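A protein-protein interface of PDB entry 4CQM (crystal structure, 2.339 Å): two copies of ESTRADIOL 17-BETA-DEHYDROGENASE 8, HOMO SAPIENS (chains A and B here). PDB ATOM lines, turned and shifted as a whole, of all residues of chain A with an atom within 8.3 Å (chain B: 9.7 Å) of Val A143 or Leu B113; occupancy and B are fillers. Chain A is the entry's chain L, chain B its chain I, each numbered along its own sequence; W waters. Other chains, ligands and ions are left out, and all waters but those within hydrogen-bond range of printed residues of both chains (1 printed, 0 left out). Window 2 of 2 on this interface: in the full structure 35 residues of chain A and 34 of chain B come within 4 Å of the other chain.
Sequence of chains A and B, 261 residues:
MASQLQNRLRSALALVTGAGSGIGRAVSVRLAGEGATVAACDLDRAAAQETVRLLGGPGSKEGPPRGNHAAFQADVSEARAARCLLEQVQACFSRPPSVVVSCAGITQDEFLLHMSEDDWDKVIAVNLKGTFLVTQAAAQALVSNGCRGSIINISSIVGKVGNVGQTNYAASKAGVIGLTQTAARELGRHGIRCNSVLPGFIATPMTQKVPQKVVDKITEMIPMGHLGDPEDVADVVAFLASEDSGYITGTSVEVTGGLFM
Among the printed residues, merely in contact across the chains: Phe A132 with Leu B112, Phe A132 with Thr B167, Ala A139 with Leu B113, Val A143 with Leu B113, Glu A186 with Phe B111, Glu A186 with Gln B166 and Leu A187 with Leu B112.
No position is printed for both chains.
Of the printed residues of chain B, Val A143 touches Leu B113.
Leu B113 touches just these residues of chain A: Ala A139, Gln A140 and Val A143.
No residue of chain B comes within 4 Å of Ser A144.
Of the printed residues of chain B, Glu A186 touches Phe B111, Leu B112, Gly B165 and Gln B166.
Of the printed residues of chain A, Gly B165 touches Glu A186 (2.5 Å).
Of the printed residues of chain A, Phe B111 touches Glu A186.
Printed residues of chain B within 4 Å of Gln A136: Leu B112 (2.8 Å) and Met B115 (2.6 Å).
Of the printed residues of chain A, Leu B112 touches Phe A132 (3.6 Å), Gln A136 (2.8 Å), Glu A186 (2.9 Å) and Leu A187 (3.9 Å).
Cys A147 touches none of the printed residues of chain B.
Gly A191 touches none of the printed residues of chain B.
The backbone carbonyl oxygen (O) of Leu B112 is in hydrogen-bond range of the side-chain amide nitrogen (NE2) of Gln A136, at 2.8 Å.
The backbone NH (N) of Leu B112 lies within hydrogen-bond range of the side-chain carboxylate (OE1) of Glu A186 (2.9 Å).
O of Leu B113 lies within hydrogen-bond range of NE2 of Gln A140 (2.8 Å).
O of Met B115 is in hydrogen-bond range of NE2 of Gln A136 (2.6 Å).
The backbone NH (N) of Gly B165 is in hydrogen-bond range of the side-chain carboxylate (OE2) of Glu A186, 2.5 Å away.
Of the 25 printed residues of chain A, 7 touch a printed residue of chain B.
Hydrophobic or aromatic side chains of chain A within 4 Å of the printed part of chain B: Phe A132, Ala A139, Val A143 and Leu A187.
Hydrophobic or aromatic side chains of chain B within 4 Å of the printed part of chain A: Leu B112, Leu B113 and Met B115.
Among the printed residues, no Asp or Glu carboxylate lies within 4 Å of a Lys or Arg side-chain nitrogen of the other chain.
Water W1 lies within hydrogen-bond range of O of Glu B110 (2.4 Å), OG1 of Thr B167 (2.6 Å), OE2 of Glu A186 (3.0 Å), N of Gln B166 (3.4 Å) and N of Leu B112 (3.4 Å).
The backbone NH (N) of Glu B110 is in hydrogen-bond range of the backbone carbonyl oxygen (O) of Gly B165 (3.0 Å).
N of Ile A192 sits at hydrogen-bond distance from O of Leu A187.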
ATOM      1  N   GLN A  90      11.782 -22.648 -30.139  1.00  0.00           N
ATOM      2  CA  GLN A  90      12.687 -23.051 -29.065  1.00  0.00           C
ATOM      3  C   GLN A  90      14.126 -23.195 -29.547  1.00  0.00           C
ATOM      4  O   GLN A  90      15.056 -23.217 -28.745  1.00  0.00           O
ATOM      5  CB  GLN A  90      12.226 -24.369 -28.443  1.00  0.00           C
ATOM      6  CG  GLN A  90      10.843 -24.337 -27.826  1.00  0.00           C
ATOM      7  CD  GLN A  90      10.360 -25.721 -27.440  1.00  0.00           C
ATOM      8  OE1 GLN A  90      10.510 -26.147 -26.295  1.00  0.00           O
ATOM      9  NE2 GLN A  90       9.785 -26.437 -28.402  1.00  0.00           N
ATOM     10  N   PRO A  96      11.165 -22.014 -24.613  1.00  0.00           N
ATOM     11  CA  PRO A  96       9.763 -22.071 -25.035  1.00  0.00           C
ATOM     12  C   PRO A  96       9.078 -20.721 -24.853  1.00  0.00           C
ATOM     13  O   PRO A  96       9.432 -19.980 -23.935  1.00  0.00           O
ATOM     14  CB  PRO A  96       9.161 -23.127 -24.107  1.00  0.00           C
ATOM     15  CG  PRO A  96       9.993 -23.046 -22.876  1.00  0.00           C
ATOM     16  CD  PRO A  96      11.389 -22.731 -23.345  1.00  0.00           C
ATOM     17  N   PHE A 132      -6.129 -26.154 -31.086  1.00  0.00           N
ATOM     18  CA  PHE A 132      -5.818 -27.269 -30.195  1.00  0.00           C
ATOM     19  C   PHE A 132      -4.349 -27.658 -30.270  1.00  0.00           C
ATOM     20  O   PHE A 132      -3.677 -27.787 -29.246  1.00  0.00           O
ATOM     21  CB  PHE A 132      -6.683 -28.485 -30.529  1.00  0.00           C
ATOM     22  CG  PHE A 132      -6.128 -29.780 -30.005  1.00  0.00           C
ATOM     23  CD1 PHE A 132      -6.118 -30.047 -28.646  1.00  0.00           C
ATOM     24  CD2 PHE A 132      -5.615 -30.730 -30.874  1.00  0.00           C
ATOM     25  CE1 PHE A 132      -5.605 -31.237 -28.161  1.00  0.00           C
ATOM     26  CE2 PHE A 132      -5.101 -31.921 -30.396  1.00  0.00           C
ATOM     27  CZ  PHE A 132      -5.097 -32.175 -29.038  1.00  0.00           C
ATOM     28  N   THR A 135      -1.999 -24.944 -28.831  1.00  0.00           N
ATOM     29  CA  THR A 135      -2.138 -24.911 -27.379  1.00  0.00           C
ATOM     30  C   THR A 135      -1.503 -26.141 -26.731  1.00  0.00           C
ATOM     31  O   THR A 135      -0.877 -26.044 -25.674  1.00  0.00           O
ATOM     32  CB  THR A 135      -3.619 -24.824 -26.962  1.00  0.00           C
ATOM     33  OG1 THR A 135      -4.238 -23.714 -27.624  1.00  0.00           O
ATOM     34  CG2 THR A 135      -3.743 -24.645 -25.456  1.00  0.00           C
ATOM     35  N   GLN A 136      -1.663 -27.294 -27.373  1.00  0.00           N
ATOM     36  CA  GLN A 136      -1.074 -28.532 -26.875  1.00  0.00           C
ATOM     37  C   GLN A 136       0.448 -28.490 -26.958  1.00  0.00           C
ATOM     38  O   GLN A 136       1.139 -28.808 -25.990  1.00  0.00           O
ATOM     39  CB  GLN A 136      -1.603 -29.735 -27.656  1.00  0.00           C
ATOM     40  CG  GLN A 136      -1.053 -31.067 -27.171  1.00  0.00           C
ATOM     41  CD  GLN A 136      -1.402 -32.218 -28.092  1.00  0.00           C
ATOM     42  OE1 GLN A 136      -1.363 -32.083 -29.315  1.00  0.00           O
ATOM     43  NE2 GLN A 136      -1.748 -33.359 -27.507  1.00  0.00           N
ATOM     44  N   ALA A 137       0.964 -28.094 -28.117  1.00  0.00           N
ATOM     45  CA  ALA A 137       2.404 -28.029 -28.335  1.00  0.00           C
ATOM     46  C   ALA A 137       3.054 -26.965 -27.456  1.00  0.00           C
ATOM     47  O   ALA A 137       4.197 -27.118 -27.022  1.00  0.00           O
ATOM     48  CB  ALA A 137       2.704 -27.758 -29.800  1.00  0.00           C
ATOM     49  N   ALA A 138       2.320 -25.887 -27.197  1.00  0.00           N
ATOM     50  CA  ALA A 138       2.815 -24.811 -26.349  1.00  0.00           C
ATOM     51  C   ALA A 138       2.970 -25.282 -24.910  1.00  0.00           C
ATOM     52  O   ALA A 138       3.988 -25.027 -24.267  1.00  0.00           O
ATOM     53  CB  ALA A 138       1.885 -23.615 -26.414  1.00  0.00           C
ATOM     54  N   ALA A 139       1.947 -25.972 -24.414  1.00  0.00           N
ATOM     55  CA  ALA A 139       1.952 -26.490 -23.052  1.00  0.00           C
ATOM     56  C   ALA A 139       3.070 -27.506 -22.854  1.00  0.00           C
ATOM     57  O   ALA A 139       3.763 -27.486 -21.837  1.00  0.00           O
ATOM     58  CB  ALA A 139       0.608 -27.114 -22.724  1.00  0.00           C
ATOM     59  N   GLN A 140       3.240 -28.387 -23.835  1.00  0.00           N
ATOM     60  CA  GLN A 140       4.275 -29.414 -23.784  1.00  0.00           C
ATOM     61  C   GLN A 140       5.669 -28.803 -23.687  1.00  0.00           C
ATOM     62  O   GLN A 140       6.530 -29.312 -22.973  1.00  0.00           O
ATOM     63  CB  GLN A 140       4.187 -30.322 -25.011  1.00  0.00           C
ATOM     64  CG  GLN A 140       2.959 -31.215 -25.038  1.00  0.00           C
ATOM     65  CD  GLN A 140       2.797 -31.939 -26.358  1.00  0.00           C
ATOM     66  OE1 GLN A 140       3.383 -31.548 -27.368  1.00  0.00           O
ATOM     67  NE2 GLN A 140       2.003 -33.004 -26.360  1.00  0.00           N
ATOM     68  N   ALA A 141       5.882 -27.707 -24.407  1.00  0.00           N
ATOM     69  CA  ALA A 141       7.174 -27.033 -24.409  1.00  0.00           C
ATOM     70  C   ALA A 141       7.421 -26.308 -23.090  1.00  0.00           C
ATOM     71  O   ALA A 141       8.567 -26.099 -22.691  1.00  0.00           O
ATOM     72  CB  ALA A 141       7.262 -26.059 -25.574  1.00  0.00           C
ATOM     73  N   LEU A 142       6.339 -25.927 -22.418  1.00  0.00           N
ATOM     74  CA  LEU A 142       6.435 -25.202 -21.157  1.00  0.00           C
ATOM     75  C   LEU A 142       6.569 -26.150 -19.968  1.00  0.00           C
ATOM     76  O   LEU A 142       7.271 -25.850 -19.002  1.00  0.00           O
ATOM     77  CB  LEU A 142       5.218 -24.294 -20.972  1.00  0.00           C
ATOM     78  CG  LEU A 142       5.149 -23.065 -21.879  1.00  0.00           C
ATOM     79  CD1 LEU A 142       3.843 -22.312 -21.672  1.00  0.00           C
ATOM     80  CD2 LEU A 142       6.342 -22.154 -21.633  1.00  0.00           C
ATOM     81  N   VAL A 143       5.893 -27.292 -20.044  1.00  0.00           N
ATOM     82  CA  VAL A 143       5.958 -28.289 -18.982  1.00  0.00           C
ATOM     83  C   VAL A 143       7.310 -29.000 -18.993  1.00  0.00           C
ATOM     84  O   VAL A 143       7.893 -29.265 -17.940  1.00  0.00           O
ATOM     85  CB  VAL A 143       4.820 -29.325 -19.110  1.00  0.00           C
ATOM     86  CG1 VAL A 143       5.019 -30.472 -18.132  1.00  0.00           C
ATOM     87  CG2 VAL A 143       3.472 -28.659 -18.883  1.00  0.00           C
ATOM     88  N   SER A 144       7.809 -29.292 -20.191  1.00  0.00           N
ATOM     89  CA  SER A 144       9.086 -29.981 -20.349  1.00  0.00           C
ATOM     90  C   SER A 144      10.250 -29.167 -19.787  1.00  0.00           C
ATOM     91  O   SER A 144      11.204 -29.726 -19.247  1.00  0.00           O
ATOM     92  CB  SER A 144       9.342 -30.300 -21.822  1.00  0.00           C
ATOM     93  OG  SER A 144      10.614 -30.900 -22.001  1.00  0.00           O
ATOM     94  N   ASN A 145      10.167 -27.847 -19.919  1.00  0.00           N
ATOM     95  CA  ASN A 145      11.210 -26.963 -19.410  1.00  0.00           C
ATOM     96  C   ASN A 145      10.891 -26.443 -18.014  1.00  0.00           C
ATOM     97  O   ASN A 145      11.666 -25.685 -17.432  1.00  0.00           O
ATOM     98  CB  ASN A 145      11.429 -25.789 -20.366  1.00  0.00           C
ATOM     99  CG  ASN A 145      12.030 -26.219 -21.689  1.00  0.00           C
ATOM    100  OD1 ASN A 145      13.251 -26.292 -21.835  1.00  0.00           O
ATOM    101  ND2 ASN A 145      11.174 -26.507 -22.662  1.00  0.00           N
ATOM    102  N   GLY A 146       9.745 -26.857 -17.482  1.00  0.00           N
ATOM    103  CA  GLY A 146       9.321 -26.440 -16.159  1.00  0.00           C
ATOM    104  C   GLY A 146       9.043 -24.952 -16.083  1.00  0.00           C
ATOM    105  O   GLY A 146       9.175 -24.341 -15.023  1.00  0.00           O
ATOM    106  N   CYS A 147       8.656 -24.369 -17.212  1.00  0.00           N
ATOM    107  CA  CYS A 147       8.380 -22.938 -17.278  1.00  0.00           C
ATOM    108  C   CYS A 147       6.881 -22.654 -17.281  1.00  0.00           C
ATOM    109  O   CYS A 147       6.129 -23.236 -18.062  1.00  0.00           O
ATOM    110  CB  CYS A 147       9.032 -22.324 -18.519  1.00  0.00           C
ATOM    111  SG  CYS A 147      10.840 -22.376 -18.524  1.00  0.00           S
ATOM    112  N   ARG A 148       6.455 -21.755 -16.398  1.00  0.00           N
ATOM    113  CA  ARG A 148       5.065 -21.319 -16.351  1.00  0.00           C
ATOM    114  C   ARG A 148       4.790 -20.376 -17.519  1.00  0.00           C
ATOM    115  O   ARG A 148       5.722 -19.919 -18.183  1.00  0.00           O
ATOM    116  CB  ARG A 148       4.758 -20.635 -15.017  1.00  0.00           C
ATOM    117  CG  ARG A 148       5.456 -19.296 -14.832  1.00  0.00           C
ATOM    118  CD  ARG A 148       5.282 -18.756 -13.417  1.00  0.00           C
ATOM    119  NE  ARG A 148       6.015 -19.546 -12.432  1.00  0.00           N
ATOM    120  CZ  ARG A 148       6.272 -19.143 -11.192  1.00  0.00           C
ATOM    121  NH1 ARG A 148       5.860 -17.951 -10.779  1.00  0.00           N
ATOM    122  NH2 ARG A 148       6.947 -19.928 -10.363  1.00  0.00           N
ATOM    123  N   GLY A 149       3.519 -20.084 -17.775  1.00  0.00           N
ATOM    124  CA  GLY A 149       3.171 -19.211 -18.880  1.00  0.00           C
ATOM    125  C   GLY A 149       1.702 -18.858 -18.989  1.00  0.00           C
ATOM    126  O   GLY A 149       0.913 -19.116 -18.079  1.00  0.00           O
ATOM    127  N   ILE A 151      -1.458 -18.941 -22.004  1.00  0.00           N
ATOM    128  CA  ILE A 151      -1.938 -19.270 -23.340  1.00  0.00           C
ATOM    129  C   ILE A 151      -3.235 -18.528 -23.643  1.00  0.00           C
ATOM    130  O   ILE A 151      -4.195 -18.592 -22.875  1.00  0.00           O
ATOM    131  CB  ILE A 151      -2.161 -20.781 -23.503  1.00  0.00           C
ATOM    132  CG1 ILE A 151      -0.877 -21.542 -23.168  1.00  0.00           C
ATOM    133  CG2 ILE A 151      -2.626 -21.101 -24.914  1.00  0.00           C
ATOM    134  CD1 ILE A 151      -0.992 -23.042 -23.323  1.00  0.00           C
ATOM    135  N   GLU A 186      -6.372 -28.186 -16.525  1.00  0.00           N
ATOM    136  CA  GLU A 186      -5.336 -29.215 -16.531  1.00  0.00           C
ATOM    137  C   GLU A 186      -3.939 -28.625 -16.357  1.00  0.00           C
ATOM    138  O   GLU A 186      -3.059 -29.257 -15.774  1.00  0.00           O
ATOM    139  CB  GLU A 186      -5.391 -30.025 -17.827  1.00  0.00           C
ATOM    140  CG  GLU A 186      -6.647 -30.862 -17.995  1.00  0.00           C
ATOM    141  CD  GLU A 186      -6.572 -31.777 -19.203  1.00  0.00           C
ATOM    142  OE1 GLU A 186      -5.497 -31.836 -19.836  1.00  0.00           O
ATOM    143  OE2 GLU A 186      -7.584 -32.437 -19.518  1.00  0.00           O
ATOM    144  N   LEU A 187      -3.742 -27.412 -16.866  1.00  0.00           N
ATOM    145  CA  LEU A 187      -2.426 -26.779 -16.846  1.00  0.00           C
ATOM    146  C   LEU A 187      -2.251 -25.829 -15.666  1.00  0.00           C
ATOM    147  O   LEU A 187      -1.227 -25.154 -15.552  1.00  0.00           O
ATOM    148  CB  LEU A 187      -2.185 -26.024 -18.153  1.00  0.00           C
ATOM    149  CG  LEU A 187      -2.226 -26.866 -19.429  1.00  0.00           C
ATOM    150  CD1 LEU A 187      -2.128 -25.976 -20.656  1.00  0.00           C
ATOM    151  CD2 LEU A 187      -1.114 -27.903 -19.421  1.00  0.00           C
ATOM    152  N   ARG A 189      -1.832 -26.602 -12.574  1.00  0.00           N
ATOM    153  CA  ARG A 189      -0.810 -27.121 -11.671  1.00  0.00           C
ATOM    154  C   ARG A 189       0.599 -26.811 -12.170  1.00  0.00           C
ATOM    155  O   ARG A 189       1.555 -26.821 -11.395  1.00  0.00           O
ATOM    156  CB  ARG A 189      -0.978 -28.630 -11.490  1.00  0.00           C
ATOM    157  CG  ARG A 189      -2.245 -29.031 -10.752  1.00  0.00           C
ATOM    158  CD  ARG A 189      -2.166 -28.663  -9.278  1.00  0.00           C
ATOM    159  NE  ARG A 189      -1.152 -29.443  -8.574  1.00  0.00           N
ATOM    160  CZ  ARG A 189      -0.856 -29.296  -7.286  1.00  0.00           C
ATOM    161  NH1 ARG A 189      -1.495 -28.394  -6.555  1.00  0.00           N
ATOM    162  NH2 ARG A 189       0.081 -30.052  -6.730  1.00  0.00           N
ATOM    163  N   HIS A 190       0.721 -26.538 -13.464  1.00  0.00           N
ATOM    164  CA  HIS A 190       2.021 -26.261 -14.061  1.00  0.00           C
ATOM    165  C   HIS A 190       2.231 -24.765 -14.280  1.00  0.00           C
ATOM    166  O   HIS A 190       3.153 -24.352 -14.982  1.00  0.00           O
ATOM    167  CB  HIS A 190       2.171 -27.016 -15.383  1.00  0.00           C
ATOM    168  CG  HIS A 190       1.996 -28.498 -15.253  1.00  0.00           C
ATOM    169  ND1 HIS A 190       0.807 -29.135 -15.530  1.00  0.00           N
ATOM    170  CD2 HIS A 190       2.859 -29.467 -14.863  1.00  0.00           C
ATOM    171  CE1 HIS A 190       0.945 -30.433 -15.323  1.00  0.00           C
ATOM    172  NE2 HIS A 190       2.181 -30.659 -14.917  1.00  0.00           N
ATOM    173  N   GLY A 191       1.367 -23.958 -13.671  1.00  0.00           N
ATOM    174  CA  GLY A 191       1.487 -22.513 -13.737  1.00  0.00           C
ATOM    175  C   GLY A 191       1.190 -21.928 -15.104  1.00  0.00           C
ATOM    176  O   GLY A 191       1.627 -20.824 -15.422  1.00  0.00           O
ATOM    177  N   ILE A 192       0.439 -22.666 -15.916  1.00  0.00           N
ATOM    178  CA  ILE A 192       0.098 -22.207 -17.256  1.00  0.00           C
ATOM    179  C   ILE A 192      -1.355 -21.747 -17.328  1.00  0.00           C
ATOM    180  O   ILE A 192      -2.279 -22.557 -17.249  1.00  0.00           O
ATOM    181  CB  ILE A 192       0.332 -23.309 -18.306  1.00  0.00           C
ATOM    182  CG1 ILE A 192       1.767 -23.833 -18.214  1.00  0.00           C
ATOM    183  CG2 ILE A 192       0.036 -22.785 -19.705  1.00  0.00           C
ATOM    184  CD1 ILE A 192       2.065 -24.964 -19.172  1.00  0.00           C
ATOM    185  N   GLU B 110      -8.142 -38.354 -22.492  1.00  0.00           N
ATOM    186  CA  GLU B 110      -6.695 -38.282 -22.344  1.00  0.00           C
ATOM    187  C   GLU B 110      -6.322 -36.868 -21.911  1.00  0.00           C
ATOM    188  O   GLU B 110      -7.015 -35.911 -22.252  1.00  0.00           O
ATOM    189  CB  GLU B 110      -5.986 -38.651 -23.652  1.00  0.00           C
ATOM    190  CG  GLU B 110      -4.469 -38.721 -23.552  1.00  0.00           C
ATOM    191  CD  GLU B 110      -3.995 -39.761 -22.553  1.00  0.00           C
ATOM    192  OE1 GLU B 110      -3.901 -40.949 -22.931  1.00  0.00           O
ATOM    193  OE2 GLU B 110      -3.714 -39.390 -21.395  1.00  0.00           O
ATOM    194  N   PHE B 111      -5.241 -36.736 -21.149  1.00  0.00           N
ATOM    195  CA  PHE B 111      -4.753 -35.418 -20.767  1.00  0.00           C
ATOM    196  C   PHE B 111      -4.259 -34.665 -21.998  1.00  0.00           C
ATOM    197  O   PHE B 111      -3.908 -35.277 -23.007  1.00  0.00           O
ATOM    198  CB  PHE B 111      -3.644 -35.533 -19.721  1.00  0.00           C
ATOM    199  CG  PHE B 111      -4.132 -35.977 -18.371  1.00  0.00           C
ATOM    200  CD1 PHE B 111      -4.616 -35.054 -17.458  1.00  0.00           C
ATOM    201  CD2 PHE B 111      -4.113 -37.316 -18.017  1.00  0.00           C
ATOM    202  CE1 PHE B 111      -5.068 -35.457 -16.215  1.00  0.00           C
ATOM    203  CE2 PHE B 111      -4.565 -37.725 -16.775  1.00  0.00           C
ATOM    204  CZ  PHE B 111      -5.043 -36.794 -15.873  1.00  0.00           C
ATOM    205  N   LEU B 112      -4.242 -33.338 -21.912  1.00  0.00           N
ATOM    206  CA  LEU B 112      -3.873 -32.490 -23.042  1.00  0.00           C
ATOM    207  C   LEU B 112      -2.467 -32.780 -23.556  1.00  0.00           C
ATOM    208  O   LEU B 112      -2.241 -32.854 -24.764  1.00  0.00           O
ATOM    209  CB  LEU B 112      -3.983 -31.014 -22.656  1.00  0.00           C
ATOM    210  CG  LEU B 112      -3.559 -30.009 -23.729  1.00  0.00           C
ATOM    211  CD1 LEU B 112      -4.498 -30.070 -24.923  1.00  0.00           C
ATOM    212  CD2 LEU B 112      -3.500 -28.603 -23.159  1.00  0.00           C
ATOM    213  N   LEU B 113      -1.528 -32.952 -22.632  1.00  0.00           N
ATOM    214  CA  LEU B 113      -0.129 -33.169 -22.982  1.00  0.00           C
ATOM    215  C   LEU B 113       0.103 -34.505 -23.683  1.00  0.00           C
ATOM    216  O   LEU B 113       1.125 -34.695 -24.343  1.00  0.00           O
ATOM    217  CB  LEU B 113       0.746 -33.090 -21.730  1.00  0.00           C
ATOM    218  CG  LEU B 113       0.739 -31.764 -20.968  1.00  0.00           C
ATOM    219  CD1 LEU B 113       1.617 -31.848 -19.728  1.00  0.00           C
ATOM    220  CD2 LEU B 113       1.191 -30.628 -21.869  1.00  0.00           C
ATOM    221  N   HIS B 114      -0.844 -35.425 -23.545  1.00  0.00           N
ATOM    222  CA  HIS B 114      -0.666 -36.777 -24.060  1.00  0.00           C
ATOM    223  C   HIS B 114      -1.692 -37.167 -25.124  1.00  0.00           C
ATOM    224  O   HIS B 114      -1.625 -38.263 -25.680  1.00  0.00           O
ATOM    225  CB  HIS B 114      -0.717 -37.785 -22.908  1.00  0.00           C
ATOM    226  CG  HIS B 114       0.377 -37.609 -21.900  1.00  0.00           C
ATOM    227  ND1 HIS B 114       1.530 -36.904 -22.168  1.00  0.00           N
ATOM    228  CD2 HIS B 114       0.491 -38.049 -20.625  1.00  0.00           C
ATOM    229  CE1 HIS B 114       2.309 -36.916 -21.100  1.00  0.00           C
ATOM    230  NE2 HIS B 114       1.703 -37.603 -20.150  1.00  0.00           N
ATOM    231  N   MET B 115      -2.636 -36.275 -25.411  1.00  0.00           N
ATOM    232  CA  MET B 115      -3.695 -36.582 -26.370  1.00  0.00           C
ATOM    233  C   MET B 115      -3.175 -36.632 -27.805  1.00  0.00           C
ATOM    234  O   MET B 115      -2.594 -35.666 -28.300  1.00  0.00           O
ATOM    235  CB  MET B 115      -4.830 -35.563 -26.266  1.00  0.00           C
ATOM    236  CG  MET B 115      -5.992 -35.847 -27.209  1.00  0.00           C
ATOM    237  SD  MET B 115      -7.386 -34.729 -26.976  1.00  0.00           S
ATOM    238  CE  MET B 115      -7.833 -35.092 -25.282  1.00  0.00           C
ATOM    239  N   SER B 116      -3.392 -37.764 -28.466  1.00  0.00           N
ATOM    240  CA  SER B 116      -2.955 -37.942 -29.844  1.00  0.00           C
ATOM    241  C   SER B 116      -3.905 -37.248 -30.813  1.00  0.00           C
ATOM    242  O   SER B 116      -4.976 -36.783 -30.422  1.00  0.00           O
ATOM    243  CB  SER B 116      -2.853 -39.429 -30.189  1.00  0.00           C
ATOM    244  OG  SER B 116      -4.132 -40.038 -30.188  1.00  0.00           O
ATOM    245  N   GLU B 117      -3.506 -37.182 -32.079  1.00  0.00           N
ATOM    246  CA  GLU B 117      -4.317 -36.537 -33.104  1.00  0.00           C
ATOM    247  C   GLU B 117      -5.561 -37.362 -33.422  1.00  0.00           C
ATOM    248  O   GLU B 117      -6.587 -36.822 -33.835  1.00  0.00           O
ATOM    249  CB  GLU B 117      -3.493 -36.310 -34.374  1.00  0.00           C
ATOM    250  CG  GLU B 117      -4.194 -35.466 -35.428  1.00  0.00           C
ATOM    251  CD  GLU B 117      -3.386 -35.330 -36.702  1.00  0.00           C
ATOM    252  OE1 GLU B 117      -2.319 -35.972 -36.805  1.00  0.00           O
ATOM    253  OE2 GLU B 117      -3.819 -34.580 -37.602  1.00  0.00           O
ATOM    254  N   ASP B 119      -7.204 -39.367 -31.154  1.00  0.00           N
ATOM    255  CA  ASP B 119      -8.123 -39.228 -30.027  1.00  0.00           C
ATOM    256  C   ASP B 119      -8.926 -37.938 -30.150  1.00  0.00           C
ATOM    257  O   ASP B 119     -10.050 -37.842 -29.656  1.00  0.00           O
ATOM    258  CB  ASP B 119      -7.363 -39.249 -28.699  1.00  0.00           C
ATOM    259  CG  ASP B 119      -6.626 -40.554 -28.468  1.00  0.00           C
ATOM    260  OD1 ASP B 119      -7.060 -41.591 -29.011  1.00  0.00           O
ATOM    261  OD2 ASP B 119      -5.610 -40.540 -27.743  1.00  0.00           O
ATOM    262  N   GLY B 165      -9.199 -34.242 -18.787  1.00  0.00           N
ATOM    263  CA  GLY B 165      -9.050 -35.395 -19.654  1.00  0.00           C
ATOM    264  C   GLY B 165     -10.038 -35.415 -20.803  1.00  0.00           C
ATOM    265  O   GLY B 165     -10.173 -36.422 -21.494  1.00  0.00           O
ATOM    266  N   GLN B 166     -10.730 -34.300 -21.011  1.00  0.00           N
ATOM    267  CA  GLN B 166     -11.718 -34.215 -22.080  1.00  0.00           C
ATOM    268  C   GLN B 166     -11.553 -32.956 -22.922  1.00  0.00           C
ATOM    269  O   GLN B 166     -12.509 -32.211 -23.127  1.00  0.00           O
ATOM    270  CB  GLN B 166     -13.134 -34.269 -21.503  1.00  0.00           C
ATOM    271  CG  GLN B 166     -13.546 -35.646 -21.009  1.00  0.00           C
ATOM    272  CD  GLN B 166     -15.014 -35.720 -20.639  1.00  0.00           C
ATOM    273  OE1 GLN B 166     -15.589 -34.755 -20.133  1.00  0.00           O
ATOM    274  NE2 GLN B 166     -15.631 -36.867 -20.895  1.00  0.00           N
ATOM    275  N   THR B 167     -10.339 -32.723 -23.412  1.00  0.00           N
ATOM    276  CA  THR B 167     -10.078 -31.594 -24.297  1.00  0.00           C
ATOM    277  C   THR B 167     -10.875 -31.746 -25.587  1.00  0.00           C
ATOM    278  O   THR B 167     -11.476 -30.791 -26.079  1.00  0.00           O
ATOM    279  CB  THR B 167      -8.579 -31.469 -24.634  1.00  0.00           C
ATOM    280  OG1 THR B 167      -7.824 -31.334 -23.424  1.00  0.00           O
ATOM    281  CG2 THR B 167      -8.328 -30.257 -25.521  1.00  0.00           C
HETATM  282  O   HOH W   1      -7.650 -33.593 -22.240  1.00  0.00           O
